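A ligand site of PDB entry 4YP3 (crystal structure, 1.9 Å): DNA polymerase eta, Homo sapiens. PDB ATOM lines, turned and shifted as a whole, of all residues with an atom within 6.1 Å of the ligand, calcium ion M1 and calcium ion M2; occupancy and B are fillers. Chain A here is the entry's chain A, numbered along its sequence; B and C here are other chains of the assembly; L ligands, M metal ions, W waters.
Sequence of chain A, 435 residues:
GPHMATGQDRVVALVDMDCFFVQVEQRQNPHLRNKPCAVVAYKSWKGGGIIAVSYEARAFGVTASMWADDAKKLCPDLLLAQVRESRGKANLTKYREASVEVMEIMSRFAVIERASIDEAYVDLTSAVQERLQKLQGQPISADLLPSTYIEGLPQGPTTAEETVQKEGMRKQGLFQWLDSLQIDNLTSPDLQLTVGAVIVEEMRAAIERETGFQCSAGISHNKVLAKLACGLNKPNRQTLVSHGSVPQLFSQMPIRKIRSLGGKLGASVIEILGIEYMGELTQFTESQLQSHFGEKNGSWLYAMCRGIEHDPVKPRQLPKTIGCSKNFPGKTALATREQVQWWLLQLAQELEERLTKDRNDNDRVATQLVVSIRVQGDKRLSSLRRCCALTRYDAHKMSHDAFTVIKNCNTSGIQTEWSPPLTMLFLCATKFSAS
The side-chain hydroxyl (OH) of Tyr 55 sits at hydrogen-bond distance from an oxygen (O12) of the ligand. O6 of 8OG 4 of chain C sits at hydrogen-bond distance from a nitrogen (N3) of the ligand. An oxygen (O12) of the ligand sits at hydrogen-bond distance from the backbone NH of Cys 19 (2.8 Å). An oxygen (O13) of the ligand is in salt-bridge range of the guanidinium group (NH1) of Arg 58, at 3.0 Å. N of Phe 20 sits at hydrogen-bond distance from O3 of the ligand. The side-chain amino group (NZ) of Lys 234 lies within salt-bridge range of an oxygen (O12) of the ligand (3.4 Å). O3 of the ligand sits at hydrogen-bond distance from N of Phe 21, at 3.1 Å.
The backbone NH (N) of Glu 119 lies within hydrogen-bond range of the side-chain hydroxyl (OG) of Ser 116 (3.2 Å). NZ of Lys 227 is in salt-bridge range of OE1 of Glu 119. O of Asp 16 sits at hydrogen-bond distance from NZ of Lys 234. O3' of DT 8 of chain B sits close to the side-chain hydroxyl (OG) of Ser 116, 3.0 Å away. The side-chain amino group (NZ) of Lys 227 lies within salt-bridge range of OP1 of DT 8 of chain B, 3.4 Å away. NH1 of Arg 58 is in hydrogen-bond range of OH of Tyr 55 (3.1 Å). The guanidinium group (NE) of Arg 58 is in hydrogen-bond range of the backbone carbonyl oxygen (O) of Val 53, 2.9 Å away. NZ of Lys 234 is in salt-bridge range of OD1 of Asp 18.
Residues that only touch the ligand: Ile 51, Asp 18, Ala 52 and DA 5 of chain C. Of the 24 residues printed, 15 come within 4 Å of the ligand. The nearest printed residue that does not touch the ligand is Ile 117 (4.04 Å).
The nearest printed residue that does not touch calcium ion M1 is Lys 234 (4.2 Å).
Ser 116 touches calcium ion M2 (OG to CA, 3.8 Å). Within 4 Å of calcium ion M2: Asp 16, Ser 116, Asp 118, Glu 119 and DT 8 of chain B. The nearest printed residue that does not touch calcium ion M2 is Lys 227 (4.7 Å).
The side-chain carboxylate (OD2) of Asp 118 binds calcium ion M1, at 2.3 Å. O11 of the ligand binds calcium ion M1 (2.3 Å). O of Met 17 is bound to calcium ion M1, 2.3 Å away. An oxygen (O8) of the ligand binds calcium ion M1, at 2.3 Å. Calcium ion M1 is bound by O5 of the ligand, at 2.4 Å. OD2 of Asp 16 binds calcium ion M1 (2.5 Å). Calcium ion M1 is bound by OD1 of Asp 16, at 2.6 Å. Calcium ion M1 has seven donor atoms within binding distance.
Calcium ion M2 is bound by the side-chain carboxylate (OE2) of Glu 119, water W9, an oxygen (O5) of the ligand, the side-chain carboxylate (OD1) of Asp 118, the side-chain carboxylate (OD1) of Asp 16 and O3' of DT 8 of chain B. Calcium ion M2 has six donor atoms within binding distance.
Water W9 lies within hydrogen-bond range of NZ of Lys 227 and O6 of the ligand. Water W3 lies within hydrogen-bond range of an oxygen (O9) of the ligand, the backbone NH of Val 53 and the guanidinium group of Arg 58. Water W10 lies within hydrogen-bond range of the backbone carbonyl oxygen (O) of Ile 51 and a nitrogen (N2) of the ligand.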
ATOM      1  N   ASP A  16      19.929  16.032 -21.346  1.00  0.00           N
ATOM      2  CA  ASP A  16      19.336  16.067 -19.994  1.00  0.00           C
ATOM      3  C   ASP A  16      20.148  15.251 -18.963  1.00  0.00           C
ATOM      4  O   ASP A  16      20.420  14.085 -19.206  1.00  0.00           O
ATOM      5  CB  ASP A  16      17.897  15.557 -20.056  1.00  0.00           C
ATOM      6  CG  ASP A  16      17.317  15.348 -18.696  1.00  0.00           C
ATOM      7  OD1 ASP A  16      16.908  16.297 -18.077  1.00  0.00           O
ATOM      8  OD2 ASP A  16      17.330  14.235 -18.215  1.00  0.00           O
ATOM      9  N   MET A  17      20.545  15.838 -17.828  1.00  0.00           N
ATOM     10  CA  MET A  17      21.442  15.139 -16.899  1.00  0.00           C
ATOM     11  C   MET A  17      20.648  14.022 -16.223  1.00  0.00           C
ATOM     12  O   MET A  17      19.446  14.203 -15.943  1.00  0.00           O
ATOM     13  CB  MET A  17      21.987  16.087 -15.809  1.00  0.00           C
ATOM     14  CG  MET A  17      22.627  17.378 -16.383  1.00  0.00           C
ATOM     15  SD  MET A  17      23.930  16.992 -17.574  1.00  0.00           S
ATOM     16  CE  MET A  17      25.059  16.105 -16.593  1.00  0.00           C
ATOM     17  N   ASP A  18      21.306  12.923 -15.922  1.00  0.00           N
ATOM     18  CA  ASP A  18      20.619  11.822 -15.242  1.00  0.00           C
ATOM     19  C   ASP A  18      20.497  12.161 -13.746  1.00  0.00           C
ATOM     20  O   ASP A  18      21.474  12.618 -13.159  1.00  0.00           O
ATOM     21  CB  ASP A  18      21.383  10.523 -15.459  1.00  0.00           C
ATOM     22  CG  ASP A  18      21.404  10.074 -16.943  1.00  0.00           C
ATOM     23  OD1 ASP A  18      20.477  10.352 -17.673  1.00  0.00           O
ATOM     24  OD2 ASP A  18      22.351   9.425 -17.366  1.00  0.00           O
ATOM     25  N   CYS A  19      19.328  11.894 -13.168  1.00  0.00           N
ATOM     26  CA  CYS A  19      19.016  12.141 -11.759  1.00  0.00           C
ATOM     27  C   CYS A  19      19.879  13.256 -11.162  1.00  0.00           C
ATOM     28  O   CYS A  19      20.734  13.020 -10.309  1.00  0.00           O
ATOM     29  CB  CYS A  19      19.146  10.827 -10.944  1.00  0.00           C
ATOM     30  SG  CYS A  19      20.679   9.842 -11.011  1.00  0.00           S
ATOM     31  N   PHE A  20      19.739  14.461 -11.700  1.00  0.00           N
ATOM     32  CA  PHE A  20      20.802  15.488 -11.612  1.00  0.00           C
ATOM     33  C   PHE A  20      21.226  15.870 -10.150  1.00  0.00           C
ATOM     34  O   PHE A  20      22.424  15.777  -9.817  1.00  0.00           O
ATOM     35  CB  PHE A  20      20.366  16.743 -12.352  1.00  0.00           C
ATOM     36  CG  PHE A  20      21.401  17.807 -12.383  1.00  0.00           C
ATOM     37  CD1 PHE A  20      22.723  17.499 -12.753  1.00  0.00           C
ATOM     38  CD2 PHE A  20      21.096  19.086 -11.942  1.00  0.00           C
ATOM     39  CE1 PHE A  20      23.729  18.498 -12.744  1.00  0.00           C
ATOM     40  CE2 PHE A  20      22.096  20.101 -11.933  1.00  0.00           C
ATOM     41  CZ  PHE A  20      23.417  19.797 -12.351  1.00  0.00           C
ATOM     42  N   PHE A  21      20.284  16.265  -9.286  1.00  0.00           N
ATOM     43  CA  PHE A  21      20.717  16.667  -7.937  1.00  0.00           C
ATOM     44  C   PHE A  21      21.427  15.489  -7.210  1.00  0.00           C
ATOM     45  O   PHE A  21      22.387  15.669  -6.441  1.00  0.00           O
ATOM     46  CB  PHE A  21      19.575  17.187  -7.060  1.00  0.00           C
ATOM     47  CG  PHE A  21      19.006  18.532  -7.496  1.00  0.00           C
ATOM     48  CD1 PHE A  21      19.315  19.095  -8.706  1.00  0.00           C
ATOM     49  CD2 PHE A  21      18.106  19.190  -6.671  1.00  0.00           C
ATOM     50  CE1 PHE A  21      18.756  20.334  -9.093  1.00  0.00           C
ATOM     51  CE2 PHE A  21      17.539  20.430  -7.038  1.00  0.00           C
ATOM     52  CZ  PHE A  21      17.872  20.990  -8.252  1.00  0.00           C
ATOM     53  N   VAL A  22      20.939  14.267  -7.462  1.00  0.00           N
ATOM     54  CA  VAL A  22      21.581  13.095  -6.894  1.00  0.00           C
ATOM     55  C   VAL A  22      23.038  13.011  -7.365  1.00  0.00           C
ATOM     56  O   VAL A  22      23.936  12.781  -6.527  1.00  0.00           O
ATOM     57  CB  VAL A  22      20.807  11.793  -7.241  1.00  0.00           C
ATOM     58  CG1 VAL A  22      21.627  10.552  -6.929  1.00  0.00           C
ATOM     59  CG2 VAL A  22      19.470  11.709  -6.441  1.00  0.00           C
ATOM     60  N   ILE A  51      13.171  15.147  -3.730  1.00  0.00           N
ATOM     61  CA  ILE A  51      13.071  15.848  -5.019  1.00  0.00           C
ATOM     62  C   ILE A  51      13.894  15.268  -6.160  1.00  0.00           C
ATOM     63  O   ILE A  51      13.724  15.695  -7.328  1.00  0.00           O
ATOM     64  CB  ILE A  51      13.420  17.315  -4.851  1.00  0.00           C
ATOM     65  CG1 ILE A  51      14.866  17.553  -4.418  1.00  0.00           C
ATOM     66  CG2 ILE A  51      12.427  17.984  -3.799  1.00  0.00           C
ATOM     67  CD1 ILE A  51      15.179  19.064  -4.422  1.00  0.00           C
ATOM     68  N   ALA A  52      14.753  14.279  -5.861  1.00  0.00           N
ATOM     69  CA  ALA A  52      15.527  13.565  -6.894  1.00  0.00           C
ATOM     70  C   ALA A  52      15.917  12.187  -6.390  1.00  0.00           C
ATOM     71  O   ALA A  52      16.193  12.013  -5.206  1.00  0.00           O
ATOM     72  CB  ALA A  52      16.791  14.357  -7.282  1.00  0.00           C
ATOM     73  N   VAL A  53      15.975  11.199  -7.292  1.00  0.00           N
ATOM     74  CA  VAL A  53      16.103   9.801  -6.885  1.00  0.00           C
ATOM     75  C   VAL A  53      17.061   9.057  -7.811  1.00  0.00           C
ATOM     76  O   VAL A  53      16.883   9.100  -9.039  1.00  0.00           O
ATOM     77  CB  VAL A  53      14.706   9.084  -6.952  1.00  0.00           C
ATOM     78  CG1 VAL A  53      14.808   7.663  -6.399  1.00  0.00           C
ATOM     79  CG2 VAL A  53      13.657   9.856  -6.190  1.00  0.00           C
ATOM     80  N   TYR A  55      18.853   5.980  -9.923  1.00  0.00           N
ATOM     81  CA  TYR A  55      18.237   4.839 -10.610  1.00  0.00           C
ATOM     82  C   TYR A  55      18.165   3.536  -9.767  1.00  0.00           C
ATOM     83  O   TYR A  55      17.142   2.813  -9.802  1.00  0.00           O
ATOM     84  CB  TYR A  55      18.951   4.608 -11.955  1.00  0.00           C
ATOM     85  CG  TYR A  55      18.460   5.668 -12.915  1.00  0.00           C
ATOM     86  CD1 TYR A  55      18.967   6.972 -12.877  1.00  0.00           C
ATOM     87  CD2 TYR A  55      17.426   5.394 -13.801  1.00  0.00           C
ATOM     88  CE1 TYR A  55      18.453   7.970 -13.727  1.00  0.00           C
ATOM     89  CE2 TYR A  55      16.916   6.383 -14.669  1.00  0.00           C
ATOM     90  CZ  TYR A  55      17.433   7.659 -14.625  1.00  0.00           C
ATOM     91  OH  TYR A  55      16.938   8.646 -15.476  1.00  0.00           O
ATOM     92  N   ARG A  58      15.151   3.952  -7.694  1.00  0.00           N
ATOM     93  CA  ARG A  58      13.943   3.827  -8.505  1.00  0.00           C
ATOM     94  C   ARG A  58      13.581   2.355  -8.673  1.00  0.00           C
ATOM     95  O   ARG A  58      12.399   2.022  -8.759  1.00  0.00           O
ATOM     96  CB  ARG A  58      14.123   4.477  -9.874  1.00  0.00           C
ATOM     97  CG  ARG A  58      14.365   5.971  -9.780  1.00  0.00           C
ATOM     98  CD  ARG A  58      14.586   6.579 -11.199  1.00  0.00           C
ATOM     99  NE  ARG A  58      15.190   7.919 -11.064  1.00  0.00           N
ATOM    100  CZ  ARG A  58      15.256   8.817 -12.014  1.00  0.00           C
ATOM    101  NH1 ARG A  58      14.753   8.564 -13.239  1.00  0.00           N
ATOM    102  NH2 ARG A  58      15.809  10.006 -11.728  1.00  0.00           N
ATOM    103  N   SER A  65       8.289  13.517  -5.137  1.00  0.00           N
ATOM    104  CA  SER A  65       6.995  13.660  -4.462  1.00  0.00           C
ATOM    105  C   SER A  65       6.578  12.441  -3.572  1.00  0.00           C
ATOM    106  O   SER A  65       5.390  12.146  -3.401  1.00  0.00           O
ATOM    107  CB  SER A  65       5.893  13.919  -5.491  1.00  0.00           C
ATOM    108  OG  SER A  65       6.292  14.915  -6.416  1.00  0.00           O
ATOM    109  N   LEU A  92      19.330  26.384  -3.331  1.00  0.00           N
ATOM    110  CA  LEU A  92      19.709  25.521  -4.447  1.00  0.00           C
ATOM    111  C   LEU A  92      21.032  25.888  -5.113  1.00  0.00           C
ATOM    112  O   LEU A  92      21.328  25.390  -6.214  1.00  0.00           O
ATOM    113  CB  LEU A  92      18.613  25.514  -5.527  1.00  0.00           C
ATOM    114  CG  LEU A  92      17.207  25.191  -4.951  1.00  0.00           C
ATOM    115  CD1 LEU A  92      16.112  25.259  -6.026  1.00  0.00           C
ATOM    116  CD2 LEU A  92      17.236  23.819  -4.349  1.00  0.00           C
ATOM    117  N   SER A 116      16.133  24.209 -18.518  1.00  0.00           N
ATOM    118  CA  SER A 116      15.865  24.012 -17.102  1.00  0.00           C
ATOM    119  C   SER A 116      17.241  24.025 -16.401  1.00  0.00           C
ATOM    120  O   SER A 116      18.279  24.148 -17.060  1.00  0.00           O
ATOM    121  CB  SER A 116      15.151  22.676 -16.846  1.00  0.00           C
ATOM    122  OG  SER A 116      16.076  21.580 -16.950  1.00  0.00           O
ATOM    123  N   ILE A 117      17.249  23.810 -15.108  1.00  0.00           N
ATOM    124  CA  ILE A 117      18.542  23.705 -14.419  1.00  0.00           C
ATOM    125  C   ILE A 117      19.431  22.513 -14.944  1.00  0.00           C
ATOM    126  O   ILE A 117      20.666  22.551 -14.801  1.00  0.00           O
ATOM    127  CB  ILE A 117      18.335  23.560 -12.889  1.00  0.00           C
ATOM    128  CG1 ILE A 117      19.627  23.940 -12.140  1.00  0.00           C
ATOM    129  CG2 ILE A 117      17.851  22.156 -12.531  1.00  0.00           C
ATOM    130  CD1 ILE A 117      19.376  24.142 -10.646  1.00  0.00           C
ATOM    131  N   ASP A 118      18.852  21.489 -15.594  1.00  0.00           N
ATOM    132  CA  ASP A 118      19.705  20.339 -15.976  1.00  0.00           C
ATOM    133  C   ASP A 118      19.517  19.898 -17.420  1.00  0.00           C
ATOM    134  O   ASP A 118      19.950  18.794 -17.798  1.00  0.00           O
ATOM    135  CB  ASP A 118      19.480  19.131 -15.046  1.00  0.00           C
ATOM    136  CG  ASP A 118      18.234  18.302 -15.448  1.00  0.00           C
ATOM    137  OD1 ASP A 118      17.219  18.906 -15.888  1.00  0.00           O
ATOM    138  OD2 ASP A 118      18.273  17.050 -15.327  1.00  0.00           O
ATOM    139  N   GLU A 119      18.933  20.761 -18.248  1.00  0.00           N
ATOM    140  CA  GLU A 119      18.840  20.442 -19.655  1.00  0.00           C
ATOM    141  C   GLU A 119      18.903  21.640 -20.617  1.00  0.00           C
ATOM    142  O   GLU A 119      18.592  22.783 -20.277  1.00  0.00           O
ATOM    143  CB  GLU A 119      17.565  19.640 -19.915  1.00  0.00           C
ATOM    144  CG  GLU A 119      16.335  20.423 -20.027  1.00  0.00           C
ATOM    145  CD  GLU A 119      15.085  19.551 -19.871  1.00  0.00           C
ATOM    146  OE1 GLU A 119      14.272  19.492 -20.798  1.00  0.00           O
ATOM    147  OE2 GLU A 119      14.886  18.911 -18.849  1.00  0.00           O
ATOM    148  N   LYS A 227      13.412  16.025 -27.347  1.00  0.00           N
ATOM    149  CA  LYS A 227      13.035  15.855 -25.948  1.00  0.00           C
ATOM    150  C   LYS A 227      12.401  14.473 -25.730  1.00  0.00           C
ATOM    151  O   LYS A 227      12.772  13.742 -24.802  1.00  0.00           O
ATOM    152  CB  LYS A 227      12.072  16.993 -25.562  1.00  0.00           C
ATOM    153  CG  LYS A 227      11.481  16.926 -24.165  1.00  0.00           C
ATOM    154  CD  LYS A 227      12.546  17.072 -23.110  1.00  0.00           C
ATOM    155  CE  LYS A 227      11.838  17.463 -21.781  1.00  0.00           C
ATOM    156  NZ  LYS A 227      12.679  17.033 -20.685  1.00  0.00           N
ATOM    157  N   LYS A 234      17.078   5.883 -21.021  1.00  0.00           N
ATOM    158  CA  LYS A 234      17.764   6.568 -19.917  1.00  0.00           C
ATOM    159  C   LYS A 234      18.086   5.473 -18.967  1.00  0.00           C
ATOM    160  O   LYS A 234      17.418   4.446 -18.984  1.00  0.00           O
ATOM    161  CB  LYS A 234      16.895   7.660 -19.229  1.00  0.00           C
ATOM    162  CG  LYS A 234      16.962   9.022 -19.849  1.00  0.00           C
ATOM    163  CD  LYS A 234      16.283  10.128 -19.030  1.00  0.00           C
ATOM    164  CE  LYS A 234      17.122  10.669 -17.870  1.00  0.00           C
ATOM    165  NZ  LYS A 234      18.190  11.722 -18.145  1.00  0.00           N
ATOM    166  N   PRO A 235      19.138   5.648 -18.150  1.00  0.00           N
ATOM    167  CA  PRO A 235      20.101   6.757 -18.108  1.00  0.00           C
ATOM    168  C   PRO A 235      21.328   6.508 -19.008  1.00  0.00           C
ATOM    169  O   PRO A 235      21.482   5.407 -19.535  1.00  0.00           O
ATOM    170  CB  PRO A 235      20.544   6.759 -16.633  1.00  0.00           C
ATOM    171  CG  PRO A 235      20.608   5.198 -16.349  1.00  0.00           C
ATOM    172  CD  PRO A 235      19.427   4.632 -17.111  1.00  0.00           C
ATOM    173  P    DT B   8       9.220  18.031 -17.732  1.00  0.00           P
ATOM    174  OP1  DT B   8      10.011  17.108 -18.578  1.00  0.00           O
ATOM    175  OP2  DT B   8       8.258  17.459 -16.718  1.00  0.00           O
ATOM    176  O5'  DT B   8      10.282  18.936 -16.892  1.00  0.00           O
ATOM    177  C5'  DT B   8      11.258  19.801 -17.562  1.00  0.00           C
ATOM    178  C4'  DT B   8      12.268  20.302 -16.538  1.00  0.00           C
ATOM    179  O4'  DT B   8      11.592  21.099 -15.585  1.00  0.00           O
ATOM    180  C3'  DT B   8      12.964  19.213 -15.758  1.00  0.00           C
ATOM    181  O3'  DT B   8      14.260  19.562 -15.630  1.00  0.00           O
ATOM    182  C2'  DT B   8      12.221  19.149 -14.434  1.00  0.00           C
ATOM    183  C1'  DT B   8      11.828  20.611 -14.276  1.00  0.00           C
ATOM    184  N1   DT B   8      10.576  20.849 -13.434  1.00  0.00           N
ATOM    185  C2   DT B   8      10.653  21.692 -12.328  1.00  0.00           C
ATOM    186  O2   DT B   8      11.675  22.262 -11.966  1.00  0.00           O
ATOM    187  N3   DT B   8       9.510  21.838 -11.654  1.00  0.00           N
ATOM    188  C4   DT B   8       8.305  21.262 -11.916  1.00  0.00           C
ATOM    189  O4   DT B   8       7.307  21.461 -11.190  1.00  0.00           O
ATOM    190  C5   DT B   8       8.265  20.387 -13.054  1.00  0.00           C
ATOM    191  C7   DT B   8       6.964  19.694 -13.403  1.00  0.00           C
ATOM    192  C6   DT B   8       9.377  20.227 -13.774  1.00  0.00           C
ATOM    193  P   8OG C   4       4.478  21.669   0.713  1.00  0.00           P
ATOM    194  OP1 8OG C   4       4.310  23.155   0.899  1.00  0.00           O
ATOM    195  OP2 8OG C   4       3.526  20.853  -0.149  1.00  0.00           O
ATOM    196  O5' 8OG C   4       5.950  21.396   0.128  1.00  0.00           O
ATOM    197  C5' 8OG C   4       7.146  21.438   0.899  1.00  0.00           C
ATOM    198  C4' 8OG C   4       8.218  22.107   0.056  1.00  0.00           C
ATOM    199  O4' 8OG C   4       8.262  21.528  -1.246  1.00  0.00           O
ATOM    200  C3' 8OG C   4       7.930  23.577  -0.184  1.00  0.00           C
ATOM    201  O3' 8OG C   4       9.209  24.161  -0.036  1.00  0.00           O
ATOM    202  C2' 8OG C   4       7.509  23.693  -1.637  1.00  0.00           C
ATOM    203  C1' 8OG C   4       8.295  22.553  -2.227  1.00  0.00           C
ATOM    204  N9  8OG C   4       7.833  22.005  -3.526  1.00  0.00           N
ATOM    205  C8  8OG C   4       6.611  21.761  -4.031  1.00  0.00           C
ATOM    206  N7  8OG C   4       6.568  21.230  -5.275  1.00  0.00           N
ATOM    207  C5  8OG C   4       7.865  21.116  -5.615  1.00  0.00           C
ATOM    208  C6  8OG C   4       8.622  20.612  -6.779  1.00  0.00           C
ATOM    209  O6  8OG C   4       8.005  20.171  -7.789  1.00  0.00           O
ATOM    210  N1  8OG C   4       9.985  20.676  -6.724  1.00  0.00           N
ATOM    211  C2  8OG C   4      10.664  21.148  -5.646  1.00  0.00           C
ATOM    212  N2  8OG C   4      12.006  21.190  -5.643  1.00  0.00           N
ATOM    213  N3  8OG C   4      10.022  21.596  -4.530  1.00  0.00           N
ATOM    214  C4  8OG C   4       8.672  21.608  -4.472  1.00  0.00           C
ATOM    215  O8  8OG C   4       5.548  22.030  -3.335  1.00  0.00           O
ATOM    216  P    DA C   5       9.487  25.704  -0.357  1.00  0.00           P
ATOM    217  OP1  DA C   5      10.320  26.089   0.769  1.00  0.00           O
ATOM    218  OP2  DA C   5       8.272  26.497  -0.657  1.00  0.00           O
ATOM    219  O5'  DA C   5      10.374  25.652  -1.689  1.00  0.00           O
ATOM    220  C5'  DA C   5      11.728  25.197  -1.645  1.00  0.00           C
ATOM    221  C4'  DA C   5      12.453  25.538  -2.938  1.00  0.00           C
ATOM    222  O4'  DA C   5      11.870  24.763  -4.038  1.00  0.00           O
ATOM    223  C3'  DA C   5      12.359  27.007  -3.364  1.00  0.00           C
ATOM    224  O3'  DA C   5      13.556  27.349  -4.104  1.00  0.00           O
ATOM    225  C2'  DA C   5      11.140  26.992  -4.272  1.00  0.00           C
ATOM    226  C1'  DA C   5      11.381  25.665  -5.027  1.00  0.00           C
ATOM    227  N9   DA C   5      10.192  25.094  -5.695  1.00  0.00           N
ATOM    228  C8   DA C   5       8.901  25.165  -5.272  1.00  0.00           C
ATOM    229  N7   DA C   5       8.038  24.586  -6.091  1.00  0.00           N
ATOM    230  C5   DA C   5       8.818  24.111  -7.124  1.00  0.00           C
ATOM    231  C6   DA C   5       8.502  23.418  -8.322  1.00  0.00           C
ATOM    232  N6   DA C   5       7.258  23.066  -8.680  1.00  0.00           N
ATOM    233  N1   DA C   5       9.515  23.090  -9.137  1.00  0.00           N
ATOM    234  C2   DA C   5      10.756  23.449  -8.795  1.00  0.00           C
ATOM    235  N3   DA C   5      11.171  24.110  -7.719  1.00  0.00           N
ATOM    236  C4   DA C   5      10.145  24.415  -6.919  1.00  0.00           C
HETATM  237  N1  LIG L   1      13.517  18.972  -9.741  1.00  0.00           N
HETATM  238  C1  LIG L   1      12.761  19.622  -8.750  1.00  0.00           C
HETATM  239  N2  LIG L   1      11.396  19.582  -8.807  1.00  0.00           N
HETATM  240  C2  LIG L   1      10.754  18.854  -9.783  1.00  0.00           C
HETATM  241  C3  LIG L   1      11.497  18.177 -10.739  1.00  0.00           C
HETATM  242  C4  LIG L   1      12.891  18.279 -10.698  1.00  0.00           C
HETATM  243  O1  LIG L   1      13.386  20.263  -7.858  1.00  0.00           O
HETATM  244  N3  LIG L   1       9.380  18.760  -9.836  1.00  0.00           N
HETATM  245  C5  LIG L   1      14.988  19.073  -9.692  1.00  0.00           C
HETATM  246  C6  LIG L   1      15.629  17.824  -9.106  1.00  0.00           C
HETATM  247  C7  LIG L   1      16.102  17.060 -10.357  1.00  0.00           C
HETATM  248  C8  LIG L   1      16.395  18.177 -11.361  1.00  0.00           C
HETATM  249  O2  LIG L   1      15.494  19.237 -11.023  1.00  0.00           O
HETATM  250  O3  LIG L   1      17.268  16.258 -10.111  1.00  0.00           O
HETATM  251  C9  LIG L   1      16.223  17.712 -12.811  1.00  0.00           C
HETATM  252  O4  LIG L   1      14.847  17.280 -12.982  1.00  0.00           O
HETATM  253  P1  LIG L   1      14.489  16.078 -13.948  1.00  0.00           P
HETATM  254  O5  LIG L   1      15.270  16.195 -15.211  1.00  0.00           O
HETATM  255  O6  LIG L   1      12.969  16.109 -14.091  1.00  0.00           O
HETATM  256  O7  LIG L   1      14.824  14.706 -13.122  1.00  0.00           O
HETATM  257  P2  LIG L   1      16.262  14.058 -12.767  1.00  0.00           P
HETATM  258  O8  LIG L   1      17.394  14.741 -13.499  1.00  0.00           O
HETATM  259  O9  LIG L   1      16.332  14.060 -11.252  1.00  0.00           O
HETATM  260  O10 LIG L   1      15.985  12.541 -13.251  1.00  0.00           O
HETATM  261  P3  LIG L   1      16.030  11.978 -14.806  1.00  0.00           P
HETATM  262  O11 LIG L   1      15.958  13.203 -15.699  1.00  0.00           O
HETATM  263  O12 LIG L   1      17.292  11.141 -14.867  1.00  0.00           O
HETATM  264  O13 LIG L   1      14.808  11.083 -14.841  1.00  0.00           O
HETATM  265 CA    CA M   1      17.287  15.055 -15.811  1.00  0.00          CA
HETATM  266 CA    CA M   2      15.393  17.811 -16.921  1.00  0.00          CA
HETATM  267  O   HOH W   1      14.935  20.662 -13.546  1.00  0.00           O
HETATM  268  O   HOH W   2      13.427  10.304 -16.778  1.00  0.00           O
HETATM  269  O   HOH W   3      15.120  12.136  -9.770  1.00  0.00           O
HETATM  270  O   HOH W   4      13.790  13.769 -17.193  1.00  0.00           O
HETATM  271  O   HOH W   5       8.376  16.820 -11.749  1.00  0.00           O
HETATM  272  O   HOH W   6      12.492  11.546 -13.524  1.00  0.00           O
HETATM  273  O   HOH W   7      11.476  14.801 -12.163  1.00  0.00           O
HETATM  274  O   HOH W   8      14.466  22.803  -7.567  1.00  0.00           O
HETATM  275  O   HOH W   9      13.528  16.550 -17.443  1.00  0.00           O
HETATM  276  O   HOH W  10      11.295  16.423  -8.159  1.00  0.00           O
